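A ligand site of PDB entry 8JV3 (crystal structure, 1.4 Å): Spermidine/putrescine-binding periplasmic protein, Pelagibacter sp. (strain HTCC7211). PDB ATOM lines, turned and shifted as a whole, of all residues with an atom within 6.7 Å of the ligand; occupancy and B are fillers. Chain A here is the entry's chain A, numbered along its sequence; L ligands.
The side-chain hydroxyl (OH) of Tyr 290 lies within hydrogen-bond range of an oxygen (O2) of the ligand (2.6 Å).
An oxygen (O2) of the ligand is in salt-bridge range of the guanidinium group (NE) of Arg 229, at 2.8 Å.
The guanidinium group of Arg 229 is in hydrogen-bond range of the backbone carbonyl oxygen of Trp 9, 3.1 Å away.
The guanidinium group (NH2) of Arg 229 sits at hydrogen-bond distance from the backbone carbonyl oxygen (O) of Gly 10, at 3.3 Å.
NE2 of Gln 17 sits at hydrogen-bond distance from OH of Tyr 13.
The side-chain hydroxyl (OH) of Tyr 112 sits close to the side-chain carboxylate (OE1) of Glu 252, 3.5 Å away.
NE1 of Trp 9 lies within hydrogen-bond range of OE2 of Glu 252.
N of Trp 9 is in hydrogen-bond range of OG1 of Thr 14, 3.5 Å away.
The side-chain carboxylate (OE2) of Glu 252 lies close to the side-chain carboxylate (OD1) of Asp 60.
The backbone carbonyl oxygen (O) of Ile 110 lies within hydrogen-bond range of the backbone NH (N) of Glu 252 (2.8 Å).
Merely in contact with the ligand: Trp 9 (3.3 Å), Tyr 13 (3.3 Å), Asp 60 (3.95 Å), Tyr 112 (3.3 Å), Trp 226 (3.4 Å) and Glu 252 (3.5 Å).
Hydrophobic or aromatic side chains that line the ligand: Trp 9, Tyr 13, Tyr 112, Trp 226 and Tyr 290.
Of the 22 residues printed, 8 come within 4 Å of the ligand.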
ATOM      1  N   SER A   8      14.867  22.877 -18.564  1.00  0.00           N
ATOM      2  CA  SER A   8      14.079  23.559 -17.554  1.00  0.00           C
ATOM      3  C   SER A   8      14.815  24.810 -17.097  1.00  0.00           C
ATOM      4  O   SER A   8      15.742  25.283 -17.764  1.00  0.00           O
ATOM      5  CB  SER A   8      13.689  22.600 -16.428  1.00  0.00           C
ATOM      6  OG  SER A   8      12.675  23.183 -15.637  1.00  0.00           O
ATOM      7  N   TRP A   9      14.407  25.365 -15.955  1.00  0.00           N
ATOM      8  CA  TRP A   9      14.657  26.777 -15.665  1.00  0.00           C
ATOM      9  C   TRP A   9      15.729  26.992 -14.608  1.00  0.00           C
ATOM     10  O   TRP A   9      16.003  28.152 -14.253  1.00  0.00           O
ATOM     11  CB  TRP A   9      13.347  27.446 -15.251  1.00  0.00           C
ATOM     12  CG  TRP A   9      12.253  27.341 -16.277  1.00  0.00           C
ATOM     13  CD1 TRP A   9      11.570  26.213 -16.655  1.00  0.00           C
ATOM     14  CD2 TRP A   9      11.684  28.418 -17.054  1.00  0.00           C
ATOM     15  NE1 TRP A   9      10.642  26.512 -17.610  1.00  0.00           N
ATOM     16  CE2 TRP A   9      10.667  27.849 -17.861  1.00  0.00           C
ATOM     17  CE3 TRP A   9      11.916  29.792 -17.130  1.00  0.00           C
ATOM     18  CZ2 TRP A   9       9.909  28.616 -18.741  1.00  0.00           C
ATOM     19  CZ3 TRP A   9      11.142  30.549 -17.997  1.00  0.00           C
ATOM     20  CH2 TRP A   9      10.145  29.956 -18.775  1.00  0.00           C
ATOM     21  N   GLY A  10      16.367  25.921 -14.149  1.00  0.00           N
ATOM     22  CA  GLY A  10      17.513  26.033 -13.285  1.00  0.00           C
ATOM     23  C   GLY A  10      17.156  26.237 -11.837  1.00  0.00           C
ATOM     24  O   GLY A  10      15.987  26.258 -11.427  1.00  0.00           O
ATOM     25  N   ALA A  12      16.296  26.454  -8.021  1.00  0.00           N
ATOM     26  CA  ALA A  12      15.427  25.668  -7.147  1.00  0.00           C
ATOM     27  C   ALA A  12      14.375  24.906  -7.924  1.00  0.00           C
ATOM     28  O   ALA A  12      13.907  23.872  -7.461  1.00  0.00           O
ATOM     29  CB  ALA A  12      14.730  26.560  -6.126  1.00  0.00           C
ATOM     30  N   TYR A  13      13.974  25.414  -9.094  1.00  0.00           N
ATOM     31  CA  TYR A  13      12.954  24.721  -9.862  1.00  0.00           C
ATOM     32  C   TYR A  13      13.488  23.418 -10.444  1.00  0.00           C
ATOM     33  O   TYR A  13      12.926  22.352 -10.221  1.00  0.00           O
ATOM     34  CB  TYR A  13      12.343  25.634 -10.937  1.00  0.00           C
ATOM     35  CG  TYR A  13      11.224  24.939 -11.685  1.00  0.00           C
ATOM     36  CD1 TYR A  13      10.117  24.472 -10.989  1.00  0.00           C
ATOM     37  CD2 TYR A  13      11.283  24.725 -13.047  1.00  0.00           C
ATOM     38  CE1 TYR A  13       9.086  23.833 -11.638  1.00  0.00           C
ATOM     39  CE2 TYR A  13      10.261  24.088 -13.706  1.00  0.00           C
ATOM     40  CZ  TYR A  13       9.156  23.637 -12.995  1.00  0.00           C
ATOM     41  OH  TYR A  13       8.115  22.987 -13.617  1.00  0.00           O
ATOM     42  N   THR A  14      14.591  23.482 -11.180  1.00  0.00           N
ATOM     43  CA  THR A  14      15.160  22.235 -11.688  1.00  0.00           C
ATOM     44  C   THR A  14      15.489  21.277 -10.552  1.00  0.00           C
ATOM     45  O   THR A  14      15.297  20.069 -10.699  1.00  0.00           O
ATOM     46  CB  THR A  14      16.396  22.504 -12.548  1.00  0.00           C
ATOM     47  OG1 THR A  14      15.978  23.139 -13.764  1.00  0.00           O
ATOM     48  CG2 THR A  14      17.154  21.206 -12.865  1.00  0.00           C
ATOM     49  N   GLN A  17      12.538  19.310  -9.566  1.00  0.00           N
ATOM     50  CA  GLN A  17      12.200  18.312 -10.573  1.00  0.00           C
ATOM     51  C   GLN A  17      13.155  17.133 -10.538  1.00  0.00           C
ATOM     52  O   GLN A  17      12.724  15.976 -10.579  1.00  0.00           O
ATOM     53  CB  GLN A  17      12.238  18.975 -11.944  1.00  0.00           C
ATOM     54  CG  GLN A  17      11.246  20.103 -12.090  1.00  0.00           C
ATOM     55  CD  GLN A  17      11.396  20.799 -13.424  1.00  0.00           C
ATOM     56  OE1 GLN A  17      12.383  21.522 -13.659  1.00  0.00           O
ATOM     57  NE2 GLN A  17      10.431  20.574 -14.310  1.00  0.00           N
ATOM     58  N   ASP A  60      10.321  21.918 -20.429  1.00  0.00           N
ATOM     59  CA  ASP A  60       9.415  22.519 -19.457  1.00  0.00           C
ATOM     60  C   ASP A  60       9.134  23.930 -19.955  1.00  0.00           C
ATOM     61  O   ASP A  60      10.052  24.740 -20.091  1.00  0.00           O
ATOM     62  CB  ASP A  60      10.109  22.535 -18.102  1.00  0.00           C
ATOM     63  CG  ASP A  60       9.231  23.086 -17.016  1.00  0.00           C
ATOM     64  OD1 ASP A  60       8.884  24.287 -17.127  1.00  0.00           O
ATOM     65  OD2 ASP A  60       8.860  22.337 -16.072  1.00  0.00           O
ATOM     66  N   VAL A  61       7.867  24.197 -20.306  1.00  0.00           N
ATOM     67  CA  VAL A  61       7.500  25.380 -21.082  1.00  0.00           C
ATOM     68  C   VAL A  61       6.339  26.135 -20.451  1.00  0.00           C
ATOM     69  O   VAL A  61       5.443  25.568 -19.832  1.00  0.00           O
ATOM     70  CB  VAL A  61       7.137  25.039 -22.540  1.00  0.00           C
ATOM     71  CG1 VAL A  61       8.364  24.590 -23.295  1.00  0.00           C
ATOM     72  CG2 VAL A  61       6.041  23.982 -22.604  1.00  0.00           C
ATOM     73  N   TYR A  62       6.367  27.451 -20.668  1.00  0.00           N
ATOM     74  CA  TYR A  62       5.211  28.297 -20.463  1.00  0.00           C
ATOM     75  C   TYR A  62       3.995  27.770 -21.218  1.00  0.00           C
ATOM     76  O   TYR A  62       4.092  27.203 -22.323  1.00  0.00           O
ATOM     77  CB  TYR A  62       5.509  29.668 -21.061  1.00  0.00           C
ATOM     78  CG  TYR A  62       6.387  30.651 -20.304  1.00  0.00           C
ATOM     79  CD1 TYR A  62       6.316  30.772 -18.921  1.00  0.00           C
ATOM     80  CD2 TYR A  62       7.231  31.508 -20.990  1.00  0.00           C
ATOM     81  CE1 TYR A  62       7.079  31.723 -18.260  1.00  0.00           C
ATOM     82  CE2 TYR A  62       7.984  32.448 -20.350  1.00  0.00           C
ATOM     83  CZ  TYR A  62       7.896  32.568 -18.983  1.00  0.00           C
ATOM     84  OH  TYR A  62       8.642  33.522 -18.316  1.00  0.00           O
ATOM     85  N   ILE A 110       3.203  21.455 -12.841  1.00  0.00           N
ATOM     86  CA  ILE A 110       2.843  22.200 -11.643  1.00  0.00           C
ATOM     87  C   ILE A 110       2.130  23.499 -12.006  1.00  0.00           C
ATOM     88  O   ILE A 110       2.127  23.956 -13.158  1.00  0.00           O
ATOM     89  CB  ILE A 110       4.049  22.454 -10.707  1.00  0.00           C
ATOM     90  CG1 ILE A 110       5.218  23.172 -11.385  1.00  0.00           C
ATOM     91  CG2 ILE A 110       4.520  21.126 -10.130  1.00  0.00           C
ATOM     92  CD1 ILE A 110       5.031  24.668 -11.647  1.00  0.00           C
ATOM     93  N   TYR A 112       2.012  27.599 -10.658  1.00  0.00           N
ATOM     94  CA  TYR A 112       2.878  28.585 -10.032  1.00  0.00           C
ATOM     95  C   TYR A 112       2.208  29.936 -10.053  1.00  0.00           C
ATOM     96  O   TYR A 112       1.229  30.152 -10.761  1.00  0.00           O
ATOM     97  CB  TYR A 112       4.212  28.680 -10.744  1.00  0.00           C
ATOM     98  CG  TYR A 112       4.212  29.156 -12.182  1.00  0.00           C
ATOM     99  CD1 TYR A 112       3.797  28.327 -13.224  1.00  0.00           C
ATOM    100  CD2 TYR A 112       4.653  30.428 -12.506  1.00  0.00           C
ATOM    101  CE1 TYR A 112       3.836  28.758 -14.537  1.00  0.00           C
ATOM    102  CE2 TYR A 112       4.725  30.862 -13.800  1.00  0.00           C
ATOM    103  CZ  TYR A 112       4.322  30.027 -14.825  1.00  0.00           C
ATOM    104  OH  TYR A 112       4.420  30.450 -16.128  1.00  0.00           O
ATOM    105  N   TRP A 114       3.015  34.212 -10.409  1.00  0.00           N
ATOM    106  CA  TRP A 114       3.774  35.450 -10.504  1.00  0.00           C
ATOM    107  C   TRP A 114       3.292  36.345  -9.357  1.00  0.00           C
ATOM    108  O   TRP A 114       2.095  36.626  -9.258  1.00  0.00           O
ATOM    109  CB  TRP A 114       3.474  36.159 -11.817  1.00  0.00           C
ATOM    110  CG  TRP A 114       3.658  35.376 -13.089  1.00  0.00           C
ATOM    111  CD1 TRP A 114       2.828  34.395 -13.569  1.00  0.00           C
ATOM    112  CD2 TRP A 114       4.681  35.557 -14.067  1.00  0.00           C
ATOM    113  NE1 TRP A 114       3.307  33.938 -14.776  1.00  0.00           N
ATOM    114  CE2 TRP A 114       4.441  34.628 -15.104  1.00  0.00           C
ATOM    115  CE3 TRP A 114       5.799  36.391 -14.161  1.00  0.00           C
ATOM    116  CZ2 TRP A 114       5.257  34.533 -16.229  1.00  0.00           C
ATOM    117  CZ3 TRP A 114       6.616  36.296 -15.285  1.00  0.00           C
ATOM    118  CH2 TRP A 114       6.355  35.352 -16.286  1.00  0.00           C
ATOM    119  N   GLY A 208      14.925  32.988 -13.179  1.00  0.00           N
ATOM    120  CA  GLY A 208      14.065  32.875 -12.007  1.00  0.00           C
ATOM    121  C   GLY A 208      14.751  33.190 -10.690  1.00  0.00           C
ATOM    122  O   GLY A 208      14.099  33.613  -9.732  1.00  0.00           O
ATOM    123  N   TRP A 226       8.639  34.571  -9.389  1.00  0.00           N
ATOM    124  CA  TRP A 226       7.826  33.382  -9.241  1.00  0.00           C
ATOM    125  C   TRP A 226       7.847  32.935  -7.778  1.00  0.00           C
ATOM    126  O   TRP A 226       8.900  32.894  -7.138  1.00  0.00           O
ATOM    127  CB  TRP A 226       8.301  32.270 -10.188  1.00  0.00           C
ATOM    128  CG  TRP A 226       8.201  32.695 -11.639  1.00  0.00           C
ATOM    129  CD1 TRP A 226       7.128  33.280 -12.258  1.00  0.00           C
ATOM    130  CD2 TRP A 226       9.212  32.566 -12.647  1.00  0.00           C
ATOM    131  NE1 TRP A 226       7.417  33.513 -13.576  1.00  0.00           N
ATOM    132  CE2 TRP A 226       8.689  33.096 -13.839  1.00  0.00           C
ATOM    133  CE3 TRP A 226      10.518  32.061 -12.650  1.00  0.00           C
ATOM    134  CZ2 TRP A 226       9.416  33.147 -15.027  1.00  0.00           C
ATOM    135  CZ3 TRP A 226      11.237  32.109 -13.827  1.00  0.00           C
ATOM    136  CH2 TRP A 226      10.693  32.651 -14.996  1.00  0.00           C
ATOM    137  N   ASN A 227       6.672  32.596  -7.246  1.00  0.00           N
ATOM    138  CA  ASN A 227       6.565  32.396  -5.803  1.00  0.00           C
ATOM    139  C   ASN A 227       7.498  31.322  -5.286  1.00  0.00           C
ATOM    140  O   ASN A 227       7.999  31.423  -4.165  1.00  0.00           O
ATOM    141  CB  ASN A 227       5.120  32.086  -5.405  1.00  0.00           C
ATOM    142  CG  ASN A 227       4.720  30.651  -5.724  1.00  0.00           C
ATOM    143  OD1 ASN A 227       4.435  30.307  -6.872  1.00  0.00           O
ATOM    144  ND2 ASN A 227       4.742  29.789  -4.697  1.00  0.00           N
ATOM    145  N   GLY A 228       7.752  30.270  -6.082  1.00  0.00           N
ATOM    146  CA  GLY A 228       8.620  29.202  -5.609  1.00  0.00           C
ATOM    147  C   GLY A 228      10.059  29.617  -5.463  1.00  0.00           C
ATOM    148  O   GLY A 228      10.792  29.048  -4.644  1.00  0.00           O
ATOM    149  N   ARG A 229      10.503  30.601  -6.252  1.00  0.00           N
ATOM    150  CA  ARG A 229      11.857  31.116  -6.122  1.00  0.00           C
ATOM    151  C   ARG A 229      11.996  31.926  -4.844  1.00  0.00           C
ATOM    152  O   ARG A 229      13.016  31.835  -4.143  1.00  0.00           O
ATOM    153  CB  ARG A 229      12.212  31.958  -7.348  1.00  0.00           C
ATOM    154  CG  ARG A 229      12.147  31.183  -8.657  1.00  0.00           C
ATOM    155  CD  ARG A 229      13.129  30.018  -8.691  1.00  0.00           C
ATOM    156  NE  ARG A 229      13.128  29.461 -10.047  1.00  0.00           N
ATOM    157  CZ  ARG A 229      14.198  29.299 -10.816  1.00  0.00           C
ATOM    158  NH1 ARG A 229      15.431  29.514 -10.360  1.00  0.00           N
ATOM    159  NH2 ARG A 229      14.007  28.876 -12.048  1.00  0.00           N
ATOM    160  N   TYR A 251      -0.042  28.093 -15.125  1.00  0.00           N
ATOM    161  CA  TYR A 251       0.057  26.647 -15.235  1.00  0.00           C
ATOM    162  C   TYR A 251       1.283  26.314 -16.071  1.00  0.00           C
ATOM    163  O   TYR A 251       1.450  26.897 -17.148  1.00  0.00           O
ATOM    164  CB  TYR A 251      -1.184  26.085 -15.945  1.00  0.00           C
ATOM    165  CG  TYR A 251      -2.554  26.435 -15.386  1.00  0.00           C
ATOM    166  CD1 TYR A 251      -2.734  26.954 -14.118  1.00  0.00           C
ATOM    167  CD2 TYR A 251      -3.678  26.179 -16.149  1.00  0.00           C
ATOM    168  CE1 TYR A 251      -4.017  27.259 -13.640  1.00  0.00           C
ATOM    169  CE2 TYR A 251      -4.942  26.477 -15.685  1.00  0.00           C
ATOM    170  CZ  TYR A 251      -5.107  27.018 -14.436  1.00  0.00           C
ATOM    171  OH  TYR A 251      -6.386  27.286 -13.984  1.00  0.00           O
ATOM    172  N   GLU A 252       2.094  25.378 -15.599  1.00  0.00           N
ATOM    173  CA  GLU A 252       3.306  24.979 -16.314  1.00  0.00           C
ATOM    174  C   GLU A 252       3.146  23.578 -16.885  1.00  0.00           C
ATOM    175  O   GLU A 252       2.334  22.777 -16.402  1.00  0.00           O
ATOM    176  CB  GLU A 252       4.526  25.054 -15.388  1.00  0.00           C
ATOM    177  CG  GLU A 252       5.882  25.014 -16.071  1.00  0.00           C
ATOM    178  CD  GLU A 252       6.233  26.276 -16.853  1.00  0.00           C
ATOM    179  OE1 GLU A 252       5.396  27.190 -16.918  1.00  0.00           O
ATOM    180  OE2 GLU A 252       7.380  26.342 -17.371  1.00  0.00           O
ATOM    181  N   ILE A 288       9.584  22.504  -3.382  1.00  0.00           N
ATOM    182  CA  ILE A 288       9.277  23.868  -3.783  1.00  0.00           C
ATOM    183  C   ILE A 288       7.770  24.062  -3.713  1.00  0.00           C
ATOM    184  O   ILE A 288       6.995  23.106  -3.856  1.00  0.00           O
ATOM    185  CB  ILE A 288       9.854  24.146  -5.195  1.00  0.00           C
ATOM    186  CG1 ILE A 288       9.956  25.657  -5.455  1.00  0.00           C
ATOM    187  CG2 ILE A 288       9.027  23.432  -6.269  1.00  0.00           C
ATOM    188  CD1 ILE A 288      10.824  25.980  -6.638  1.00  0.00           C
ATOM    189  N   TYR A 290       5.204  24.796  -5.445  1.00  0.00           N
ATOM    190  CA  TYR A 290       4.432  24.758  -6.683  1.00  0.00           C
ATOM    191  C   TYR A 290       3.491  23.563  -6.579  1.00  0.00           C
ATOM    192  O   TYR A 290       3.869  22.498  -6.101  1.00  0.00           O
ATOM    193  CB  TYR A 290       5.332  24.610  -7.932  1.00  0.00           C
ATOM    194  CG  TYR A 290       6.187  25.841  -8.250  1.00  0.00           C
ATOM    195  CD1 TYR A 290       5.736  27.126  -7.971  1.00  0.00           C
ATOM    196  CD2 TYR A 290       7.449  25.718  -8.837  1.00  0.00           C
ATOM    197  CE1 TYR A 290       6.488  28.236  -8.268  1.00  0.00           C
ATOM    198  CE2 TYR A 290       8.221  26.837  -9.134  1.00  0.00           C
ATOM    199  CZ  TYR A 290       7.735  28.090  -8.836  1.00  0.00           C
ATOM    200  OH  TYR A 290       8.483  29.208  -9.116  1.00  0.00           O
HETATM  201  N1  LIG L   1       8.631  28.442 -13.977  1.00  0.00           N
HETATM  202  C1  LIG L   1       8.908  28.733 -12.528  1.00  0.00           C
HETATM  203  C2  LIG L   1      10.360  28.676 -12.049  1.00  0.00           C
HETATM  204  O1  LIG L   1      11.312  28.515 -12.850  1.00  0.00           O
HETATM  205  O2  LIG L   1      10.481  28.820 -10.810  1.00  0.00           O
HETATM  206  C3  LIG L   1       9.154  27.093 -14.355  1.00  0.00           C
HETATM  207  C4  LIG L   1       9.265  29.481 -14.847  1.00  0.00           C
HETATM  208  C5  LIG L   1       7.153  28.458 -14.178  1.00  0.00           C
